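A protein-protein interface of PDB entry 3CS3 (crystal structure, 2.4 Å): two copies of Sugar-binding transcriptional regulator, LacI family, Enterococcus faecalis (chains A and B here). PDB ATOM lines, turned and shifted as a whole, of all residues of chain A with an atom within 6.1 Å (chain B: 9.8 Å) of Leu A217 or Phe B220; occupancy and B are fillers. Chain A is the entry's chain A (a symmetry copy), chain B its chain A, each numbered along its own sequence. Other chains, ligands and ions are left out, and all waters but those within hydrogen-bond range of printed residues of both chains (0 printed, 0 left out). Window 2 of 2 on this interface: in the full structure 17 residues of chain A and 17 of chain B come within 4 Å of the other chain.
Among the printed residues, pairs that only touch across the chains: Glu A216 with Leu B217 (3.6 Å), Leu A217 with Glu B216 (3.6 Å), Phe A220 with Leu B217 (3.7 Å) and Leu A217 with Phe B220 (3.7 Å).
Lys A194 touches Glu B216, and with the chains exchanged Glu A216 touches Lys B194.
Glu A216 touches Leu B217, and with the chains exchanged Leu A217 touches Glu B216.
Leu A217 touches Phe B220, and with the chains exchanged Phe A220 touches Leu B217.
Phe A220 touches its own counterpart, Phe B220.
No residue of chain B comes within 4 Å of Ser A215.
Glu A216 touches two residues of chain B.
Of chain B, only Glu B216 and Phe B220 come within 4 Å of Leu A217.
No residue of chain B comes within 4 Å of Ala A219.
Of the printed residues of chain B, Phe A220 touches Leu B217 and Phe B220.
No residue of chain B comes within 4 Å of Val A221.
Gly B20 touches none of the printed residues of chain A.
Printed residues of chain A within 4 Å of Lys B194: Glu A216 (3.0 Å).
Printed residues of chain A within 4 Å of Leu B217: Glu A216 (3.6 Å) and Phe A220 (3.7 Å).
Phe B220 touches just these residues of chain A: Leu A217 (3.7 Å) and Phe A220 (3.3 Å).
The nearest residue of chain A that does not touch Phe B220 is Val A221 (4.1 Å).
The side-chain amino group (NZ) of Lys A194 is in salt-bridge range of the side-chain carboxylate (OE2) of Glu A160 (3.0 Å).
Of the 21 printed residues of chain B, 4 touch a printed residue of chain A.
Printed residues of chain B that touch a printed residue of chain A: Lys B194, Glu B216, Leu B217 and Phe B220.
Of the 11 printed residues of chain A, 4 touch a printed residue of chain B.
Printed residues of chain A that touch a printed residue of chain B: Lys A194, Glu A216, Leu A217 and Phe A220.
Among the printed residues, Asp or Glu carboxylates within 4 Å of a Lys or Arg side-chain nitrogen of the other chain: Lys A194 with Glu B216 (3.0 Å) and Glu A216 with Lys B194 (3.0 Å).
NZ of Lys A194 lies within salt-bridge range of OE2 of Glu B216.
NZ of Lys B194 lies within salt-bridge range of OE2 of Glu A216 (3.0 Å).
The backbone carbonyl oxygen (O) of Phe A220 sits close to the backbone carbonyl oxygen (O) of Phe B220 (3.3 Å).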
ATOM      1  N   GLU A 160     -27.581  18.447  23.711  1.00  0.00           N
ATOM      2  CA  GLU A 160     -27.584  18.020  22.307  1.00  0.00           C
ATOM      3  C   GLU A 160     -28.977  17.773  21.663  1.00  0.00           C
ATOM      4  O   GLU A 160     -29.179  18.176  20.510  1.00  0.00           O
ATOM      5  CB  GLU A 160     -26.636  16.820  22.131  1.00  0.00           C
ATOM      6  CG  GLU A 160     -26.543  16.237  20.732  1.00  0.00           C
ATOM      7  CD  GLU A 160     -25.582  15.068  20.649  1.00  0.00           C
ATOM      8  OE1 GLU A 160     -24.424  15.203  21.103  1.00  0.00           O
ATOM      9  OE2 GLU A 160     -25.983  14.011  20.118  1.00  0.00           O
ATOM     10  N   ILE A 190     -23.338  20.107  17.972  1.00  0.00           N
ATOM     11  CA  ILE A 190     -23.243  18.687  17.593  1.00  0.00           C
ATOM     12  C   ILE A 190     -24.626  18.123  17.252  1.00  0.00           C
ATOM     13  O   ILE A 190     -24.769  17.355  16.300  1.00  0.00           O
ATOM     14  CB  ILE A 190     -22.515  17.825  18.674  1.00  0.00           C
ATOM     15  CG1 ILE A 190     -21.035  18.226  18.799  1.00  0.00           C
ATOM     16  CG2 ILE A 190     -22.644  16.312  18.391  1.00  0.00           C
ATOM     17  CD1 ILE A 190     -20.210  18.121  17.513  1.00  0.00           C
ATOM     18  N   LYS A 194     -25.912  16.382  13.769  1.00  0.00           N
ATOM     19  CA  LYS A 194     -26.731  15.165  13.726  1.00  0.00           C
ATOM     20  C   LYS A 194     -27.876  15.238  12.718  1.00  0.00           C
ATOM     21  O   LYS A 194     -28.016  14.347  11.879  1.00  0.00           O
ATOM     22  CB  LYS A 194     -27.281  14.819  15.114  1.00  0.00           C
ATOM     23  CG  LYS A 194     -26.642  13.607  15.775  1.00  0.00           C
ATOM     24  CD  LYS A 194     -25.335  13.928  16.495  1.00  0.00           C
ATOM     25  CE  LYS A 194     -24.755  12.663  17.126  1.00  0.00           C
ATOM     26  NZ  LYS A 194     -23.872  12.938  18.292  1.00  0.00           N
ATOM     27  N   SER A 215     -15.213  21.470  22.748  1.00  0.00           N
ATOM     28  CA  SER A 215     -15.302  20.055  23.051  1.00  0.00           C
ATOM     29  C   SER A 215     -14.340  19.302  22.144  1.00  0.00           C
ATOM     30  O   SER A 215     -14.091  19.727  21.008  1.00  0.00           O
ATOM     31  CB  SER A 215     -16.732  19.551  22.848  1.00  0.00           C
ATOM     32  OG  SER A 215     -17.129  19.584  21.487  1.00  0.00           O
ATOM     33  N   GLU A 216     -13.791  18.196  22.640  1.00  0.00           N
ATOM     34  CA  GLU A 216     -12.856  17.419  21.829  1.00  0.00           C
ATOM     35  C   GLU A 216     -13.541  16.690  20.675  1.00  0.00           C
ATOM     36  O   GLU A 216     -12.908  16.455  19.652  1.00  0.00           O
ATOM     37  CB  GLU A 216     -11.961  16.497  22.670  1.00  0.00           C
ATOM     38  CG  GLU A 216     -12.662  15.372  23.422  1.00  0.00           C
ATOM     39  CD  GLU A 216     -11.681  14.500  24.202  1.00  0.00           C
ATOM     40  OE1 GLU A 216     -12.084  13.932  25.240  1.00  0.00           O
ATOM     41  OE2 GLU A 216     -10.508  14.378  23.779  1.00  0.00           O
ATOM     42  N   LEU A 217     -14.829  16.370  20.821  1.00  0.00           N
ATOM     43  CA  LEU A 217     -15.605  15.811  19.705  1.00  0.00           C
ATOM     44  C   LEU A 217     -15.688  16.796  18.536  1.00  0.00           C
ATOM     45  O   LEU A 217     -15.552  16.399  17.377  1.00  0.00           O
ATOM     46  CB  LEU A 217     -17.006  15.386  20.153  1.00  0.00           C
ATOM     47  CG  LEU A 217     -17.946  14.782  19.098  1.00  0.00           C
ATOM     48  CD1 LEU A 217     -17.342  13.555  18.407  1.00  0.00           C
ATOM     49  CD2 LEU A 217     -19.303  14.438  19.710  1.00  0.00           C
ATOM     50  N   GLY A 218     -15.869  18.079  18.853  1.00  0.00           N
ATOM     51  CA  GLY A 218     -15.895  19.151  17.856  1.00  0.00           C
ATOM     52  C   GLY A 218     -14.618  19.275  17.047  1.00  0.00           C
ATOM     53  O   GLY A 218     -14.653  19.700  15.886  1.00  0.00           O
ATOM     54  N   ALA A 219     -13.498  18.888  17.660  1.00  0.00           N
ATOM     55  CA  ALA A 219     -12.193  18.866  16.995  1.00  0.00           C
ATOM     56  C   ALA A 219     -12.015  17.737  15.971  1.00  0.00           C
ATOM     57  O   ALA A 219     -11.173  17.844  15.071  1.00  0.00           O
ATOM     58  CB  ALA A 219     -11.069  18.835  18.028  1.00  0.00           C
ATOM     59  N   PHE A 220     -12.805  16.672  16.099  1.00  0.00           N
ATOM     60  CA  PHE A 220     -12.636  15.477  15.262  1.00  0.00           C
ATOM     61  C   PHE A 220     -13.796  15.235  14.296  1.00  0.00           C
ATOM     62  O   PHE A 220     -13.737  14.338  13.446  1.00  0.00           O
ATOM     63  CB  PHE A 220     -12.390  14.237  16.133  1.00  0.00           C
ATOM     64  CG  PHE A 220     -11.046  14.228  16.803  1.00  0.00           C
ATOM     65  CD1 PHE A 220      -9.918  13.768  16.126  1.00  0.00           C
ATOM     66  CD2 PHE A 220     -10.901  14.689  18.106  1.00  0.00           C
ATOM     67  CE1 PHE A 220      -8.667  13.770  16.744  1.00  0.00           C
ATOM     68  CE2 PHE A 220      -9.663  14.695  18.733  1.00  0.00           C
ATOM     69  CZ  PHE A 220      -8.540  14.234  18.051  1.00  0.00           C
ATOM     70  N   VAL A 221     -14.839  16.050  14.429  1.00  0.00           N
ATOM     71  CA  VAL A 221     -16.041  15.941  13.605  1.00  0.00           C
ATOM     72  C   VAL A 221     -15.765  16.494  12.192  1.00  0.00           C
ATOM     73  O   VAL A 221     -14.751  17.174  11.979  1.00  0.00           O
ATOM     74  CB  VAL A 221     -17.248  16.621  14.330  1.00  0.00           C
ATOM     75  CG1 VAL A 221     -17.194  18.136  14.210  1.00  0.00           C
ATOM     76  CG2 VAL A 221     -18.582  16.060  13.861  1.00  0.00           C
ATOM     77  N   GLN A 222     -16.636  16.182  11.231  1.00  0.00           N
ATOM     78  CA  GLN A 222     -16.411  16.558   9.833  1.00  0.00           C
ATOM     79  C   GLN A 222     -17.470  17.531   9.295  1.00  0.00           C
ATOM     80  O   GLN A 222     -18.639  17.154   9.134  1.00  0.00           O
ATOM     81  CB  GLN A 222     -16.358  15.309   8.949  1.00  0.00           C
ATOM     82  CG  GLN A 222     -15.194  15.288   7.975  1.00  0.00           C
ATOM     83  CD  GLN A 222     -13.925  14.735   8.605  1.00  0.00           C
ATOM     84  OE1 GLN A 222     -12.937  15.452   8.774  1.00  0.00           O
ATOM     85  NE2 GLN A 222     -13.952  13.454   8.965  1.00  0.00           N
ATOM     86  N   GLY B  20     -17.522   8.318  31.077  1.00  0.00           N
ATOM     87  CA  GLY B  20     -18.233   9.439  30.456  1.00  0.00           C
ATOM     88  C   GLY B  20     -18.347   9.326  28.947  1.00  0.00           C
ATOM     89  O   GLY B  20     -19.039  10.119  28.305  1.00  0.00           O
ATOM     90  N   SER B  21     -17.664   8.328  28.391  1.00  0.00           N
ATOM     91  CA  SER B  21     -17.752   8.001  26.982  1.00  0.00           C
ATOM     92  C   SER B  21     -19.025   7.195  26.688  1.00  0.00           C
ATOM     93  O   SER B  21     -19.447   7.086  25.532  1.00  0.00           O
ATOM     94  CB  SER B  21     -16.496   7.239  26.543  1.00  0.00           C
ATOM     95  OG  SER B  21     -16.705   5.835  26.504  1.00  0.00           O
ATOM     96  N   GLU B  25     -25.437   8.457  27.340  1.00  0.00           N
ATOM     97  CA  GLU B  25     -26.481   7.668  26.696  1.00  0.00           C
ATOM     98  C   GLU B  25     -27.042   6.583  27.625  1.00  0.00           C
ATOM     99  O   GLU B  25     -28.182   6.142  27.461  1.00  0.00           O
ATOM    100  CB  GLU B  25     -26.003   7.109  25.345  1.00  0.00           C
ATOM    101  CG  GLU B  25     -24.516   6.739  25.274  1.00  0.00           C
ATOM    102  CD  GLU B  25     -23.603   7.892  24.857  1.00  0.00           C
ATOM    103  OE1 GLU B  25     -23.825   8.473  23.774  1.00  0.00           O
ATOM    104  OE2 GLU B  25     -22.647   8.201  25.605  1.00  0.00           O
ATOM    105  N   ASP B 186     -12.581   2.071  25.554  1.00  0.00           N
ATOM    106  CA  ASP B 186     -12.275   3.088  24.546  1.00  0.00           C
ATOM    107  C   ASP B 186     -11.487   4.273  25.094  1.00  0.00           C
ATOM    108  O   ASP B 186     -10.679   4.853  24.386  1.00  0.00           O
ATOM    109  CB  ASP B 186     -13.563   3.603  23.894  1.00  0.00           C
ATOM    110  CG  ASP B 186     -13.984   2.788  22.671  1.00  0.00           C
ATOM    111  OD1 ASP B 186     -13.517   1.640  22.492  1.00  0.00           O
ATOM    112  OD2 ASP B 186     -14.793   3.307  21.875  1.00  0.00           O
ATOM    113  N   ILE B 190      -8.110   5.765  23.736  1.00  0.00           N
ATOM    114  CA  ILE B 190      -7.927   7.177  23.361  1.00  0.00           C
ATOM    115  C   ILE B 190      -6.650   7.744  23.989  1.00  0.00           C
ATOM    116  O   ILE B 190      -5.918   8.497  23.345  1.00  0.00           O
ATOM    117  CB  ILE B 190      -9.177   8.054  23.694  1.00  0.00           C
ATOM    118  CG1 ILE B 190     -10.387   7.646  22.835  1.00  0.00           C
ATOM    119  CG2 ILE B 190      -8.885   9.562  23.536  1.00  0.00           C
ATOM    120  CD1 ILE B 190     -10.178   7.723  21.319  1.00  0.00           C
ATOM    121  N   TYR B 193      -3.906   6.640  21.763  1.00  0.00           N
ATOM    122  CA  TYR B 193      -3.891   7.588  20.633  1.00  0.00           C
ATOM    123  C   TYR B 193      -3.130   8.874  20.963  1.00  0.00           C
ATOM    124  O   TYR B 193      -2.321   9.338  20.158  1.00  0.00           O
ATOM    125  CB  TYR B 193      -5.310   7.967  20.212  1.00  0.00           C
ATOM    126  CG  TYR B 193      -5.967   7.058  19.208  1.00  0.00           C
ATOM    127  CD1 TYR B 193      -6.416   5.789  19.569  1.00  0.00           C
ATOM    128  CD2 TYR B 193      -6.175   7.481  17.902  1.00  0.00           C
ATOM    129  CE1 TYR B 193      -7.038   4.956  18.647  1.00  0.00           C
ATOM    130  CE2 TYR B 193      -6.797   6.658  16.971  1.00  0.00           C
ATOM    131  CZ  TYR B 193      -7.225   5.398  17.352  1.00  0.00           C
ATOM    132  OH  TYR B 193      -7.843   4.579  16.439  1.00  0.00           O
ATOM    133  N   LYS B 194      -3.398   9.432  22.145  1.00  0.00           N
ATOM    134  CA  LYS B 194      -2.740  10.653  22.622  1.00  0.00           C
ATOM    135  C   LYS B 194      -1.215  10.569  22.601  1.00  0.00           C
ATOM    136  O   LYS B 194      -0.558  11.446  22.039  1.00  0.00           O
ATOM    137  CB  LYS B 194      -3.221  11.027  24.029  1.00  0.00           C
ATOM    138  CG  LYS B 194      -4.128  12.247  24.094  1.00  0.00           C
ATOM    139  CD  LYS B 194      -5.592  11.930  23.800  1.00  0.00           C
ATOM    140  CE  LYS B 194      -6.435  13.202  23.880  1.00  0.00           C
ATOM    141  NZ  LYS B 194      -7.865  12.943  24.197  1.00  0.00           N
ATOM    142  N   ASN B 214     -17.574   1.515  22.418  1.00  0.00           N
ATOM    143  CA  ASN B 214     -18.056   2.262  21.247  1.00  0.00           C
ATOM    144  C   ASN B 214     -18.385   3.731  21.568  1.00  0.00           C
ATOM    145  O   ASN B 214     -19.496   4.208  21.343  1.00  0.00           O
ATOM    146  CB  ASN B 214     -19.232   1.528  20.580  1.00  0.00           C
ATOM    147  CG  ASN B 214     -19.632   2.124  19.239  1.00  0.00           C
ATOM    148  OD1 ASN B 214     -18.795   2.593  18.466  1.00  0.00           O
ATOM    149  ND2 ASN B 214     -20.929   2.107  18.962  1.00  0.00           N
ATOM    150  N   SER B 215     -17.399   4.434  22.114  1.00  0.00           N
ATOM    151  CA  SER B 215     -17.519   5.855  22.377  1.00  0.00           C
ATOM    152  C   SER B 215     -17.656   6.585  21.050  1.00  0.00           C
ATOM    153  O   SER B 215     -17.111   6.138  20.032  1.00  0.00           O
ATOM    154  CB  SER B 215     -16.296   6.366  23.143  1.00  0.00           C
ATOM    155  OG  SER B 215     -15.111   6.309  22.367  1.00  0.00           O
ATOM    156  N   GLU B 216     -18.389   7.696  21.050  1.00  0.00           N
ATOM    157  CA  GLU B 216     -18.568   8.452  19.813  1.00  0.00           C
ATOM    158  C   GLU B 216     -17.293   9.166  19.367  1.00  0.00           C
ATOM    159  O   GLU B 216     -17.108   9.378  18.174  1.00  0.00           O
ATOM    160  CB  GLU B 216     -19.789   9.384  19.855  1.00  0.00           C
ATOM    161  CG  GLU B 216     -19.737  10.526  20.861  1.00  0.00           C
ATOM    162  CD  GLU B 216     -20.984  11.406  20.801  1.00  0.00           C
ATOM    163  OE1 GLU B 216     -21.348  11.994  21.842  1.00  0.00           O
ATOM    164  OE2 GLU B 216     -21.600  11.511  19.716  1.00  0.00           O
ATOM    165  N   LEU B 217     -16.407   9.497  20.309  1.00  0.00           N
ATOM    166  CA  LEU B 217     -15.088  10.040  19.954  1.00  0.00           C
ATOM    167  C   LEU B 217     -14.272   9.035  19.137  1.00  0.00           C
ATOM    168  O   LEU B 217     -13.620   9.410  18.162  1.00  0.00           O
ATOM    169  CB  LEU B 217     -14.311  10.483  21.197  1.00  0.00           C
ATOM    170  CG  LEU B 217     -12.907  11.074  20.995  1.00  0.00           C
ATOM    171  CD1 LEU B 217     -12.908  12.284  20.055  1.00  0.00           C
ATOM    172  CD2 LEU B 217     -12.270  11.438  22.335  1.00  0.00           C
ATOM    173  N   GLY B 218     -14.349   7.759  19.519  1.00  0.00           N
ATOM    174  CA  GLY B 218     -13.689   6.670  18.797  1.00  0.00           C
ATOM    175  C   GLY B 218     -14.135   6.523  17.355  1.00  0.00           C
ATOM    176  O   GLY B 218     -13.357   6.078  16.502  1.00  0.00           O
ATOM    177  N   ALA B 219     -15.382   6.914  17.087  1.00  0.00           N
ATOM    178  CA  ALA B 219     -15.943   6.915  15.733  1.00  0.00           C
ATOM    179  C   ALA B 219     -15.405   8.024  14.818  1.00  0.00           C
ATOM    180  O   ALA B 219     -15.462   7.896  13.590  1.00  0.00           O
ATOM    181  CB  ALA B 219     -17.467   6.957  15.788  1.00  0.00           C
ATOM    182  N   PHE B 220     -14.881   9.097  15.410  1.00  0.00           N
ATOM    183  CA  PHE B 220     -14.458  10.276  14.643  1.00  0.00           C
ATOM    184  C   PHE B 220     -12.947  10.508  14.657  1.00  0.00           C
ATOM    185  O   PHE B 220     -12.434  11.389  13.957  1.00  0.00           O
ATOM    186  CB  PHE B 220     -15.203  11.530  15.123  1.00  0.00           C
ATOM    187  CG  PHE B 220     -16.660  11.541  14.759  1.00  0.00           C
ATOM    188  CD1 PHE B 220     -17.075  11.981  13.504  1.00  0.00           C
ATOM    189  CD2 PHE B 220     -17.619  11.103  15.664  1.00  0.00           C
ATOM    190  CE1 PHE B 220     -18.428  11.982  13.162  1.00  0.00           C
ATOM    191  CE2 PHE B 220     -18.968  11.100  15.337  1.00  0.00           C
ATOM    192  CZ  PHE B 220     -19.375  11.541  14.081  1.00  0.00           C
ATOM    193  N   VAL B 221     -12.246   9.703  15.450  1.00  0.00           N
ATOM    194  CA  VAL B 221     -10.796   9.804  15.603  1.00  0.00           C
ATOM    195  C   VAL B 221     -10.091   9.223  14.359  1.00  0.00           C
ATOM    196  O   VAL B 221     -10.728   8.535  13.551  1.00  0.00           O
ATOM    197  CB  VAL B 221     -10.354   9.146  16.950  1.00  0.00           C
ATOM    198  CG1 VAL B 221     -10.326   7.628  16.851  1.00  0.00           C
ATOM    199  CG2 VAL B 221      -9.031   9.706  17.450  1.00  0.00           C
ATOM    200  N   GLN B 222      -8.803   9.524  14.188  1.00  0.00           N
ATOM    201  CA  GLN B 222      -8.069   9.122  12.986  1.00  0.00           C
ATOM    202  C   GLN B 222      -6.920   8.146  13.282  1.00  0.00           C
ATOM    203  O   GLN B 222      -5.925   8.529  13.912  1.00  0.00           O
ATOM    204  CB  GLN B 222      -7.527  10.354  12.258  1.00  0.00           C
ATOM    205  CG  GLN B 222      -7.779  10.352  10.760  1.00  0.00           C
ATOM    206  CD  GLN B 222      -9.150  10.907  10.406  1.00  0.00           C
ATOM    207  OE1 GLN B 222     -10.015  10.186   9.906  1.00  0.00           O
ATOM    208  NE2 GLN B 222      -9.354  12.193  10.674  1.00  0.00           N
ATOM    209  N   PRO B 223      -7.051   6.878  12.835  1.00  0.00           N
ATOM    210  CA  PRO B 223      -8.196   6.260  12.152  1.00  0.00           C
ATOM    211  C   PRO B 223      -9.269   5.768  13.131  1.00  0.00           C
ATOM    212  O   PRO B 223      -9.043   5.806  14.341  1.00  0.00           O
ATOM    213  CB  PRO B 223      -7.555   5.078  11.440  1.00  0.00           C
ATOM    214  CG  PRO B 223      -6.446   4.661  12.343  1.00  0.00           C
ATOM    215  CD  PRO B 223      -5.935   5.923  12.994  1.00  0.00           C
ATOM    216  N   ARG B 224     -10.418   5.329  12.607  1.00  0.00           N
ATOM    217  CA  ARG B 224     -11.568   4.913  13.430  1.00  0.00           C
ATOM    218  C   ARG B 224     -11.207   3.758  14.363  1.00  0.00           C
ATOM    219  O   ARG B 224     -10.654   2.738  13.937  1.00  0.00           O
ATOM    220  CB  ARG B 224     -12.790   4.591  12.538  1.00  0.00           C
ATOM    221  CG  ARG B 224     -13.682   3.425  12.973  1.00  0.00           C
ATOM    222  CD  ARG B 224     -15.039   3.824  13.522  1.00  0.00           C
ATOM    223  NE  ARG B 224     -15.129   3.668  14.974  1.00  0.00           N
ATOM    224  CZ  ARG B 224     -16.253   3.400  15.643  1.00  0.00           C
ATOM    225  NH1 ARG B 224     -17.405   3.237  15.003  1.00  0.00           N
ATOM    226  NH2 ARG B 224     -16.226   3.297  16.963  1.00  0.00           N
ATOM    227  N   LEU B 225     -11.488   3.954  15.647  1.00  0.00           N
ATOM    228  CA  LEU B 225     -11.155   2.974  16.671  1.00  0.00           C
ATOM    229  C   LEU B 225     -12.079   1.764  16.594  1.00  0.00           C
ATOM    230  O   LEU B 225     -13.280   1.869  16.868  1.00  0.00           O
ATOM    231  CB  LEU B 225     -11.194   3.608  18.065  1.00  0.00           C
ATOM    232  CG  LEU B 225     -11.013   2.695  19.288  1.00  0.00           C
ATOM    233  CD1 LEU B 225      -9.651   2.011  19.302  1.00  0.00           C
ATOM    234  CD2 LEU B 225     -11.216   3.492  20.560  1.00  0.00           C
ATOM    235  N   ALA B 226     -11.503   0.628  16.195  1.00  0.00           N
ATOM    236  CA  ALA B 226     -12.180  -0.672  16.223  1.00  0.00           C
ATOM    237  C   ALA B 226     -12.529  -1.001  17.670  1.00  0.00           C
ATOM    238  O   ALA B 226     -11.726  -0.765  18.584  1.00  0.00           O
ATOM    239  CB  ALA B 226     -11.286  -1.747  15.630  1.00  0.00           C
ATOM    240  N   THR B 227     -13.732  -1.519  17.886  1.00  0.00           N
ATOM    241  CA  THR B 227     -14.290  -1.548  19.235  1.00  0.00           C
ATOM    242  C   THR B 227     -15.417  -2.553  19.386  1.00  0.00           C
ATOM    243  O   THR B 227     -15.904  -3.111  18.402  1.00  0.00           O
ATOM    244  CB  THR B 227     -14.804  -0.129  19.656  1.00  0.00           C
ATOM    245  OG1 THR B 227     -15.177  -0.134  21.038  1.00  0.00           O
ATOM    246  CG2 THR B 227     -15.998   0.306  18.791  1.00  0.00           C
